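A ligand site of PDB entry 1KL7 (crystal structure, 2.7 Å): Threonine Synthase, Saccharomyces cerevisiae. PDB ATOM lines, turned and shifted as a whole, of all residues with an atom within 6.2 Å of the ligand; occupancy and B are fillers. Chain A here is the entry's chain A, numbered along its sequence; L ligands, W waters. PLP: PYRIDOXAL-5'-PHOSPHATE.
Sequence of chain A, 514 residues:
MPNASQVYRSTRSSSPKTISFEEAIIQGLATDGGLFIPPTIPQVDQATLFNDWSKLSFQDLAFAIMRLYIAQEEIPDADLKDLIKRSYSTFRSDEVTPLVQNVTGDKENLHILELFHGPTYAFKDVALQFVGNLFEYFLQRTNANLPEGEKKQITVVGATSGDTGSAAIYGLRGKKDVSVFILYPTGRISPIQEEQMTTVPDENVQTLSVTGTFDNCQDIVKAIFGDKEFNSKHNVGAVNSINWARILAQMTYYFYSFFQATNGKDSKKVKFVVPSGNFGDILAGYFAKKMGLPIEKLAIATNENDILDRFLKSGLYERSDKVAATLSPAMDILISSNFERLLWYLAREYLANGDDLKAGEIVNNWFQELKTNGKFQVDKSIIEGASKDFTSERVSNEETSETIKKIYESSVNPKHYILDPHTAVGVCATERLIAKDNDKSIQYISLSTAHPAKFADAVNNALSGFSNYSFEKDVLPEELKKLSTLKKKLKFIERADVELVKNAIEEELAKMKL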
ATOM      1  N   ALA A 122      -8.717  12.240  10.522  1.00  0.00           N
ATOM      2  CA  ALA A 122      -9.477  12.351   9.289  1.00  0.00           C
ATOM      3  C   ALA A 122      -8.449  12.375   8.165  1.00  0.00           C
ATOM      4  O   ALA A 122      -7.339  12.889   8.330  1.00  0.00           O
ATOM      5  CB  ALA A 122     -10.287  13.613   9.291  1.00  0.00           C
ATOM      6  N   PHE A 123      -8.816  11.826   7.010  1.00  0.00           N
ATOM      7  CA  PHE A 123      -7.908  11.737   5.866  1.00  0.00           C
ATOM      8  C   PHE A 123      -7.353  13.032   5.294  1.00  0.00           C
ATOM      9  O   PHE A 123      -6.366  13.005   4.570  1.00  0.00           O
ATOM     10  CB  PHE A 123      -8.565  10.902   4.746  1.00  0.00           C
ATOM     11  CG  PHE A 123      -9.138  11.719   3.619  1.00  0.00           C
ATOM     12  CD1 PHE A 123      -8.354  12.035   2.507  1.00  0.00           C
ATOM     13  CD2 PHE A 123     -10.456  12.161   3.663  1.00  0.00           C
ATOM     14  CE1 PHE A 123      -8.879  12.762   1.457  1.00  0.00           C
ATOM     15  CE2 PHE A 123     -10.995  12.900   2.624  1.00  0.00           C
ATOM     16  CZ  PHE A 123     -10.200  13.195   1.516  1.00  0.00           C
ATOM     17  N   LYS A 124      -7.947  14.166   5.598  1.00  0.00           N
ATOM     18  CA  LYS A 124      -7.427  15.404   5.040  1.00  0.00           C
ATOM     19  C   LYS A 124      -6.055  15.781   5.584  1.00  0.00           C
ATOM     20  O   LYS A 124      -5.416  16.723   5.100  1.00  0.00           O
ATOM     21  CB  LYS A 124      -8.430  16.534   5.243  1.00  0.00           C
ATOM     22  CG  LYS A 124      -9.675  16.320   4.424  1.00  0.00           C
ATOM     23  CD  LYS A 124     -10.567  17.545   4.377  1.00  0.00           C
ATOM     24  CE  LYS A 124     -11.476  17.429   3.171  1.00  0.00           C
ATOM     25  NZ  LYS A 124     -12.225  16.170   3.287  1.00  0.00           N
ATOM     26  N   ASP A 163     -15.578  19.506  10.746  1.00  0.00           N
ATOM     27  CA  ASP A 163     -14.225  18.959  10.814  1.00  0.00           C
ATOM     28  C   ASP A 163     -13.211  19.609   9.877  1.00  0.00           C
ATOM     29  O   ASP A 163     -12.074  19.866  10.286  1.00  0.00           O
ATOM     30  CB  ASP A 163     -14.264  17.436  10.546  1.00  0.00           C
ATOM     31  CG  ASP A 163     -14.801  17.086   9.154  1.00  0.00           C
ATOM     32  OD1 ASP A 163     -15.917  17.547   8.815  1.00  0.00           O
ATOM     33  OD2 ASP A 163     -14.116  16.340   8.425  1.00  0.00           O
ATOM     34  N   THR A 164     -13.611  19.862   8.643  1.00  0.00           N
ATOM     35  CA  THR A 164     -12.741  20.459   7.627  1.00  0.00           C
ATOM     36  C   THR A 164     -11.644  21.353   8.205  1.00  0.00           C
ATOM     37  O   THR A 164     -10.462  21.196   7.886  1.00  0.00           O
ATOM     38  CB  THR A 164     -13.557  21.283   6.612  1.00  0.00           C
ATOM     39  OG1 THR A 164     -14.039  22.479   7.247  1.00  0.00           O
ATOM     40  CG2 THR A 164     -14.752  20.472   6.123  1.00  0.00           C
ATOM     41  N   SER A 241      -9.804  23.702  -1.048  1.00  0.00           N
ATOM     42  CA  SER A 241      -9.802  22.260  -1.260  1.00  0.00           C
ATOM     43  C   SER A 241      -9.273  21.994  -2.667  1.00  0.00           C
ATOM     44  O   SER A 241      -9.108  20.848  -3.081  1.00  0.00           O
ATOM     45  CB  SER A 241     -11.222  21.688  -1.159  1.00  0.00           C
ATOM     46  OG  SER A 241     -11.996  22.058  -2.306  1.00  0.00           O
ATOM     47  N   ARG A 246      -2.603  19.596  -2.784  1.00  0.00           N
ATOM     48  CA  ARG A 246      -3.495  18.633  -2.180  1.00  0.00           C
ATOM     49  C   ARG A 246      -3.546  17.374  -3.034  1.00  0.00           C
ATOM     50  O   ARG A 246      -3.267  16.277  -2.551  1.00  0.00           O
ATOM     51  CB  ARG A 246      -4.910  19.199  -2.036  1.00  0.00           C
ATOM     52  CG  ARG A 246      -5.148  20.034  -0.793  1.00  0.00           C
ATOM     53  CD  ARG A 246      -6.644  20.140  -0.560  1.00  0.00           C
ATOM     54  NE  ARG A 246      -6.977  20.638   0.783  1.00  0.00           N
ATOM     55  CZ  ARG A 246      -8.099  20.339   1.437  1.00  0.00           C
ATOM     56  NH1 ARG A 246      -9.011  19.551   0.867  1.00  0.00           N
ATOM     57  NH2 ARG A 246      -8.311  20.809   2.661  1.00  0.00           N
ATOM     58  N   GLN A 250      -2.110  13.439  -2.083  1.00  0.00           N
ATOM     59  CA  GLN A 250      -3.006  12.298  -2.045  1.00  0.00           C
ATOM     60  C   GLN A 250      -2.692  11.164  -2.991  1.00  0.00           C
ATOM     61  O   GLN A 250      -3.258  10.092  -2.866  1.00  0.00           O
ATOM     62  CB  GLN A 250      -4.433  12.762  -2.245  1.00  0.00           C
ATOM     63  CG  GLN A 250      -4.850  13.722  -1.155  1.00  0.00           C
ATOM     64  CD  GLN A 250      -6.306  14.086  -1.244  1.00  0.00           C
ATOM     65  OE1 GLN A 250      -6.660  15.170  -1.707  1.00  0.00           O
ATOM     66  NE2 GLN A 250      -7.173  13.169  -0.811  1.00  0.00           N
ATOM     67  N   VAL A 274     -13.876   5.078  -3.668  1.00  0.00           N
ATOM     68  CA  VAL A 274     -13.595   6.271  -2.916  1.00  0.00           C
ATOM     69  C   VAL A 274     -14.782   7.115  -2.557  1.00  0.00           C
ATOM     70  O   VAL A 274     -15.392   7.711  -3.415  1.00  0.00           O
ATOM     71  CB  VAL A 274     -12.597   7.153  -3.715  1.00  0.00           C
ATOM     72  CG1 VAL A 274     -12.218   8.391  -2.925  1.00  0.00           C
ATOM     73  CG2 VAL A 274     -11.391   6.347  -4.089  1.00  0.00           C
ATOM     74  N   PRO A 275     -15.133   7.178  -1.262  1.00  0.00           N
ATOM     75  CA  PRO A 275     -16.290   8.025  -0.964  1.00  0.00           C
ATOM     76  C   PRO A 275     -15.847   9.454  -1.324  1.00  0.00           C
ATOM     77  O   PRO A 275     -14.866   9.963  -0.783  1.00  0.00           O
ATOM     78  CB  PRO A 275     -16.484   7.799   0.551  1.00  0.00           C
ATOM     79  CG  PRO A 275     -15.105   7.446   1.015  1.00  0.00           C
ATOM     80  CD  PRO A 275     -14.565   6.569  -0.044  1.00  0.00           C
ATOM     81  N   SER A 276     -16.574  10.096  -2.243  1.00  0.00           N
ATOM     82  CA  SER A 276     -16.172  11.419  -2.722  1.00  0.00           C
ATOM     83  C   SER A 276     -17.061  12.606  -2.431  1.00  0.00           C
ATOM     84  O   SER A 276     -18.273  12.464  -2.265  1.00  0.00           O
ATOM     85  CB  SER A 276     -15.948  11.333  -4.210  1.00  0.00           C
ATOM     86  OG  SER A 276     -15.120  10.219  -4.543  1.00  0.00           O
ATOM     87  N   GLY A 277     -16.451  13.785  -2.401  1.00  0.00           N
ATOM     88  CA  GLY A 277     -17.169  15.025  -2.178  1.00  0.00           C
ATOM     89  C   GLY A 277     -16.754  15.973  -3.298  1.00  0.00           C
ATOM     90  O   GLY A 277     -17.433  16.081  -4.328  1.00  0.00           O
ATOM     91  N   ASN A 278     -15.630  16.638  -3.108  1.00  0.00           N
ATOM     92  CA  ASN A 278     -15.111  17.556  -4.106  1.00  0.00           C
ATOM     93  C   ASN A 278     -14.198  16.921  -5.151  1.00  0.00           C
ATOM     94  O   ASN A 278     -13.546  17.633  -5.909  1.00  0.00           O
ATOM     95  CB  ASN A 278     -14.378  18.717  -3.437  1.00  0.00           C
ATOM     96  CG  ASN A 278     -15.323  19.681  -2.786  1.00  0.00           C
ATOM     97  OD1 ASN A 278     -16.347  20.077  -3.373  1.00  0.00           O
ATOM     98  ND2 ASN A 278     -14.997  20.077  -1.560  1.00  0.00           N
ATOM     99  N   PHE A 279     -14.142  15.588  -5.164  1.00  0.00           N
ATOM    100  CA  PHE A 279     -13.364  14.846  -6.168  1.00  0.00           C
ATOM    101  C   PHE A 279     -11.840  14.840  -6.069  1.00  0.00           C
ATOM    102  O   PHE A 279     -11.169  14.094  -6.800  1.00  0.00           O
ATOM    103  CB  PHE A 279     -13.758  15.328  -7.583  1.00  0.00           C
ATOM    104  CG  PHE A 279     -13.728  14.251  -8.627  1.00  0.00           C
ATOM    105  CD1 PHE A 279     -14.658  13.212  -8.600  1.00  0.00           C
ATOM    106  CD2 PHE A 279     -12.791  14.279  -9.655  1.00  0.00           C
ATOM    107  CE1 PHE A 279     -14.671  12.234  -9.585  1.00  0.00           C
ATOM    108  CE2 PHE A 279     -12.796  13.299 -10.646  1.00  0.00           C
ATOM    109  CZ  PHE A 279     -13.740  12.282 -10.609  1.00  0.00           C
ATOM    110  N   GLY A 280     -11.284  15.648  -5.174  1.00  0.00           N
ATOM    111  CA  GLY A 280      -9.831  15.699  -5.046  1.00  0.00           C
ATOM    112  C   GLY A 280      -9.189  14.371  -4.729  1.00  0.00           C
ATOM    113  O   GLY A 280      -8.196  13.970  -5.331  1.00  0.00           O
ATOM    114  N   ASP A 281      -9.774  13.657  -3.769  1.00  0.00           N
ATOM    115  CA  ASP A 281      -9.265  12.367  -3.350  1.00  0.00           C
ATOM    116  C   ASP A 281      -9.217  11.373  -4.483  1.00  0.00           C
ATOM    117  O   ASP A 281      -8.167  10.806  -4.787  1.00  0.00           O
ATOM    118  CB  ASP A 281     -10.164  11.818  -2.249  1.00  0.00           C
ATOM    119  CG  ASP A 281      -9.551  10.640  -1.518  1.00  0.00           C
ATOM    120  OD1 ASP A 281     -10.237  10.081  -0.632  1.00  0.00           O
ATOM    121  OD2 ASP A 281      -8.387  10.286  -1.810  1.00  0.00           O
ATOM    122  N   ILE A 282     -10.354  11.161  -5.146  1.00  0.00           N
ATOM    123  CA  ILE A 282     -10.401  10.197  -6.244  1.00  0.00           C
ATOM    124  C   ILE A 282      -9.640  10.699  -7.465  1.00  0.00           C
ATOM    125  O   ILE A 282      -9.099   9.891  -8.222  1.00  0.00           O
ATOM    126  CB  ILE A 282     -11.847   9.856  -6.642  1.00  0.00           C
ATOM    127  CG1 ILE A 282     -11.856   8.522  -7.364  1.00  0.00           C
ATOM    128  CG2 ILE A 282     -12.422  10.907  -7.566  1.00  0.00           C
ATOM    129  CD1 ILE A 282     -13.246   7.883  -7.475  1.00  0.00           C
ATOM    130  N   ALA A 330     -19.438  15.424   5.540  1.00  0.00           N
ATOM    131  CA  ALA A 330     -18.280  15.924   4.782  1.00  0.00           C
ATOM    132  C   ALA A 330     -18.330  15.737   3.254  1.00  0.00           C
ATOM    133  O   ALA A 330     -17.438  16.191   2.538  1.00  0.00           O
ATOM    134  CB  ALA A 330     -16.997  15.315   5.347  1.00  0.00           C
ATOM    135  N   MET A 331     -19.358  15.064   2.762  1.00  0.00           N
ATOM    136  CA  MET A 331     -19.493  14.850   1.324  1.00  0.00           C
ATOM    137  C   MET A 331     -20.735  15.561   0.829  1.00  0.00           C
ATOM    138  O   MET A 331     -21.039  15.549  -0.352  1.00  0.00           O
ATOM    139  CB  MET A 331     -19.604  13.361   1.023  1.00  0.00           C
ATOM    140  CG  MET A 331     -18.300  12.613   1.194  1.00  0.00           C
ATOM    141  SD  MET A 331     -18.636  10.763   1.535  1.00  0.00           S
ATOM    142  CE  MET A 331     -19.774  10.373   0.014  1.00  0.00           C
ATOM    143  N   SER A 336     -18.908  19.558  -6.928  1.00  0.00           N
ATOM    144  CA  SER A 336     -17.615  18.938  -6.662  1.00  0.00           C
ATOM    145  C   SER A 336     -16.479  19.739  -7.302  1.00  0.00           C
ATOM    146  O   SER A 336     -16.094  19.453  -8.433  1.00  0.00           O
ATOM    147  CB  SER A 336     -17.629  17.515  -7.227  1.00  0.00           C
ATOM    148  OG  SER A 336     -16.463  16.807  -6.913  1.00  0.00           O
ATOM    149  N   ASN A 338     -13.070  19.960  -7.549  1.00  0.00           N
ATOM    150  CA  ASN A 338     -11.973  19.426  -8.357  1.00  0.00           C
ATOM    151  C   ASN A 338     -12.411  18.715  -9.608  1.00  0.00           C
ATOM    152  O   ASN A 338     -11.605  18.450 -10.509  1.00  0.00           O
ATOM    153  CB  ASN A 338     -11.120  18.476  -7.534  1.00  0.00           C
ATOM    154  CG  ASN A 338     -10.300  19.189  -6.528  1.00  0.00           C
ATOM    155  OD1 ASN A 338      -9.295  19.799  -6.877  1.00  0.00           O
ATOM    156  ND2 ASN A 338     -10.716  19.144  -5.283  1.00  0.00           N
ATOM    157  N   ASP A 420     -16.790   4.492  10.126  1.00  0.00           N
ATOM    158  CA  ASP A 420     -17.365   5.815  10.275  1.00  0.00           C
ATOM    159  C   ASP A 420     -18.357   5.857   9.082  1.00  0.00           C
ATOM    160  O   ASP A 420     -18.215   5.100   8.128  1.00  0.00           O
ATOM    161  CB  ASP A 420     -16.282   6.884  10.129  1.00  0.00           C
ATOM    162  CG  ASP A 420     -16.485   7.765   8.894  1.00  0.00           C
ATOM    163  OD1 ASP A 420     -17.276   8.729   8.971  1.00  0.00           O
ATOM    164  OD2 ASP A 420     -15.852   7.483   7.837  1.00  0.00           O
ATOM    165  N   HIS A 422     -18.735   7.952   6.524  1.00  0.00           N
ATOM    166  CA  HIS A 422     -18.147   8.291   5.222  1.00  0.00           C
ATOM    167  C   HIS A 422     -17.495   7.050   4.583  1.00  0.00           C
ATOM    168  O   HIS A 422     -17.639   6.811   3.368  1.00  0.00           O
ATOM    169  CB  HIS A 422     -17.127   9.404   5.365  1.00  0.00           C
ATOM    170  CG  HIS A 422     -17.691  10.675   5.948  1.00  0.00           C
ATOM    171  ND1 HIS A 422     -17.970  10.816   7.289  1.00  0.00           N
ATOM    172  CD2 HIS A 422     -18.002  11.859   5.376  1.00  0.00           C
ATOM    173  CE1 HIS A 422     -18.434  12.035   7.517  1.00  0.00           C
ATOM    174  NE2 HIS A 422     -18.458  12.685   6.371  1.00  0.00           N
ATOM    175  N   THR A 449     -11.913   7.394   5.222  1.00  0.00           N
ATOM    176  CA  THR A 449     -11.580   8.794   5.364  1.00  0.00           C
ATOM    177  C   THR A 449     -11.689   9.397   6.749  1.00  0.00           C
ATOM    178  O   THR A 449     -11.217  10.500   6.974  1.00  0.00           O
ATOM    179  CB  THR A 449     -12.447   9.595   4.401  1.00  0.00           C
ATOM    180  OG1 THR A 449     -13.830   9.410   4.764  1.00  0.00           O
ATOM    181  CG2 THR A 449     -12.248   9.084   2.986  1.00  0.00           C
ATOM    182  N   ALA A 450     -12.332   8.685   7.665  1.00  0.00           N
ATOM    183  CA  ALA A 450     -12.479   9.208   9.015  1.00  0.00           C
ATOM    184  C   ALA A 450     -12.551   8.105  10.047  1.00  0.00           C
ATOM    185  O   ALA A 450     -13.117   7.049   9.806  1.00  0.00           O
ATOM    186  CB  ALA A 450     -13.709  10.068   9.117  1.00  0.00           C
ATOM    187  N   PHE A 455     -17.414  10.704  14.228  1.00  0.00           N
ATOM    188  CA  PHE A 455     -18.850  10.733  13.960  1.00  0.00           C
ATOM    189  C   PHE A 455     -19.544   9.678  14.803  1.00  0.00           C
ATOM    190  O   PHE A 455     -20.025   8.659  14.306  1.00  0.00           O
ATOM    191  CB  PHE A 455     -19.111  10.513  12.443  1.00  0.00           C
ATOM    192  CG  PHE A 455     -18.395  11.514  11.571  1.00  0.00           C
ATOM    193  CD1 PHE A 455     -17.108  11.248  11.095  1.00  0.00           C
ATOM    194  CD2 PHE A 455     -18.952  12.760  11.328  1.00  0.00           C
ATOM    195  CE1 PHE A 455     -16.394  12.219  10.389  1.00  0.00           C
ATOM    196  CE2 PHE A 455     -18.238  13.741  10.621  1.00  0.00           C
ATOM    197  CZ  PHE A 455     -16.959  13.466  10.152  1.00  0.00           C
HETATM  198  N1  PLP L   1     -14.729  12.012   3.946  1.00  0.00           N
HETATM  199  C2  PLP L   1     -14.290  12.791   5.007  1.00  0.00           C
HETATM  200  C2A PLP L   1     -14.272  12.103   6.347  1.00  0.00           C
HETATM  201  C3  PLP L   1     -13.902  14.158   4.716  1.00  0.00           C
HETATM  202  O3  PLP L   1     -13.511  14.863   5.826  1.00  0.00           O
HETATM  203  C4  PLP L   1     -13.980  14.629   3.384  1.00  0.00           C
HETATM  204  C4A PLP L   1     -13.556  15.990   3.191  1.00  0.00           C
HETATM  205  C5  PLP L   1     -14.461  13.712   2.292  1.00  0.00           C
HETATM  206  C6  PLP L   1     -14.828  12.417   2.631  1.00  0.00           C
HETATM  207  C5A PLP L   1     -14.441  14.224   0.784  1.00  0.00           C
HETATM  208  O4P PLP L   1     -13.178  14.071   0.010  1.00  0.00           O
HETATM  209  P   PLP L   1     -12.968  14.840  -1.494  1.00  0.00           P
HETATM  210  O1P PLP L   1     -11.529  15.013  -1.684  1.00  0.00           O
HETATM  211  O2P PLP L   1     -13.513  16.237  -1.254  1.00  0.00           O
HETATM  212  O3P PLP L   1     -13.690  14.039  -2.488  1.00  0.00           O
HETATM  213  O   HOH W   1     -11.785  17.265  -2.909  1.00  0.00           O
HETATM  214  O   HOH W   2     -12.234  11.602   0.009  1.00  0.00           O
HETATM  215  O   HOH W   3     -12.805  11.730  -4.403  1.00  0.00           O
HETATM  216  O   HOH W   4     -11.114  14.731   6.616  1.00  0.00           O
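OG1 of Thr 449 lies within hydrogen-bond range of N1 of the ligand. An oxygen (O3P) of the ligand is in hydrogen-bond range of the backbone NH of Gly 277. The backbone NH (N) of Phe 279 sits at hydrogen-bond distance from an oxygen (O3P) of the ligand, at 3.1 Å. The side-chain amino group (NZ) of Lys 124 is bonded to a carbon (C4A) of the ligand, at 1.3 Å. N of Asp 281 lies within hydrogen-bond range of O1P of the ligand, 3.0 Å away. The backbone NH (N) of Asn 278 sits at hydrogen-bond distance from an oxygen (O2P) of the ligand (2.8 Å). The side-chain carboxylate of Asp 163 lies within hydrogen-bond range of an oxygen (O3) of the ligand, 3.0 Å away.
N of Phe 279 lies within hydrogen-bond range of OG of Ser 336, 3.2 Å away. The backbone carbonyl oxygen (O) of Asn 278 is in hydrogen-bond range of the backbone NH (N) of Asn 338. NE2 of Gln 250 sits at hydrogen-bond distance from OD2 of Asp 281 (3.3 Å). The backbone NH (N) of Phe 123 is in hydrogen-bond range of the backbone carbonyl oxygen (O) of Thr 449, at 2.7 Å. O of Gly 277 sits at hydrogen-bond distance from OG of Ser 336, 2.9 Å away. The side-chain hydroxyl of Ser 276 sits at hydrogen-bond distance from the backbone carbonyl oxygen of Val 274, 2.8 Å away. ND1 of His 422 is in hydrogen-bond range of OD1 of Asp 420 (2.8 Å). OG of Ser 336 lies close to O of Asn 278, 3.2 Å away.
Merely in contact with the ligand: Ala 330, Phe 123, Ala 450, Gly 280, His 422, Ser 276 and Met 331. 14 residues have an atom within 4 Å of the ligand: Phe 123, Lys 124, Asp 163, Ser 276, Gly 277, Asn 278, Phe 279, Gly 280, Asp 281, Ala 330, Met 331, His 422, Thr 449 and Ala 450. The nearest printed residue that does not touch the ligand is Pro 275 (4.2 Å).
Water W4 lies within hydrogen-bond range of an oxygen (O3) of the ligand (2.5 Å) and the backbone NH (N) of Lys 124 (3.4 Å). Water W1 lies within hydrogen-bond range of O1P of the ligand, N of Gly 280, ND2 of Asn 338 and O of Asn 278. Water W3 lies within hydrogen-bond range of N of Ile 282, OG of Ser 276 and O3P of the ligand.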
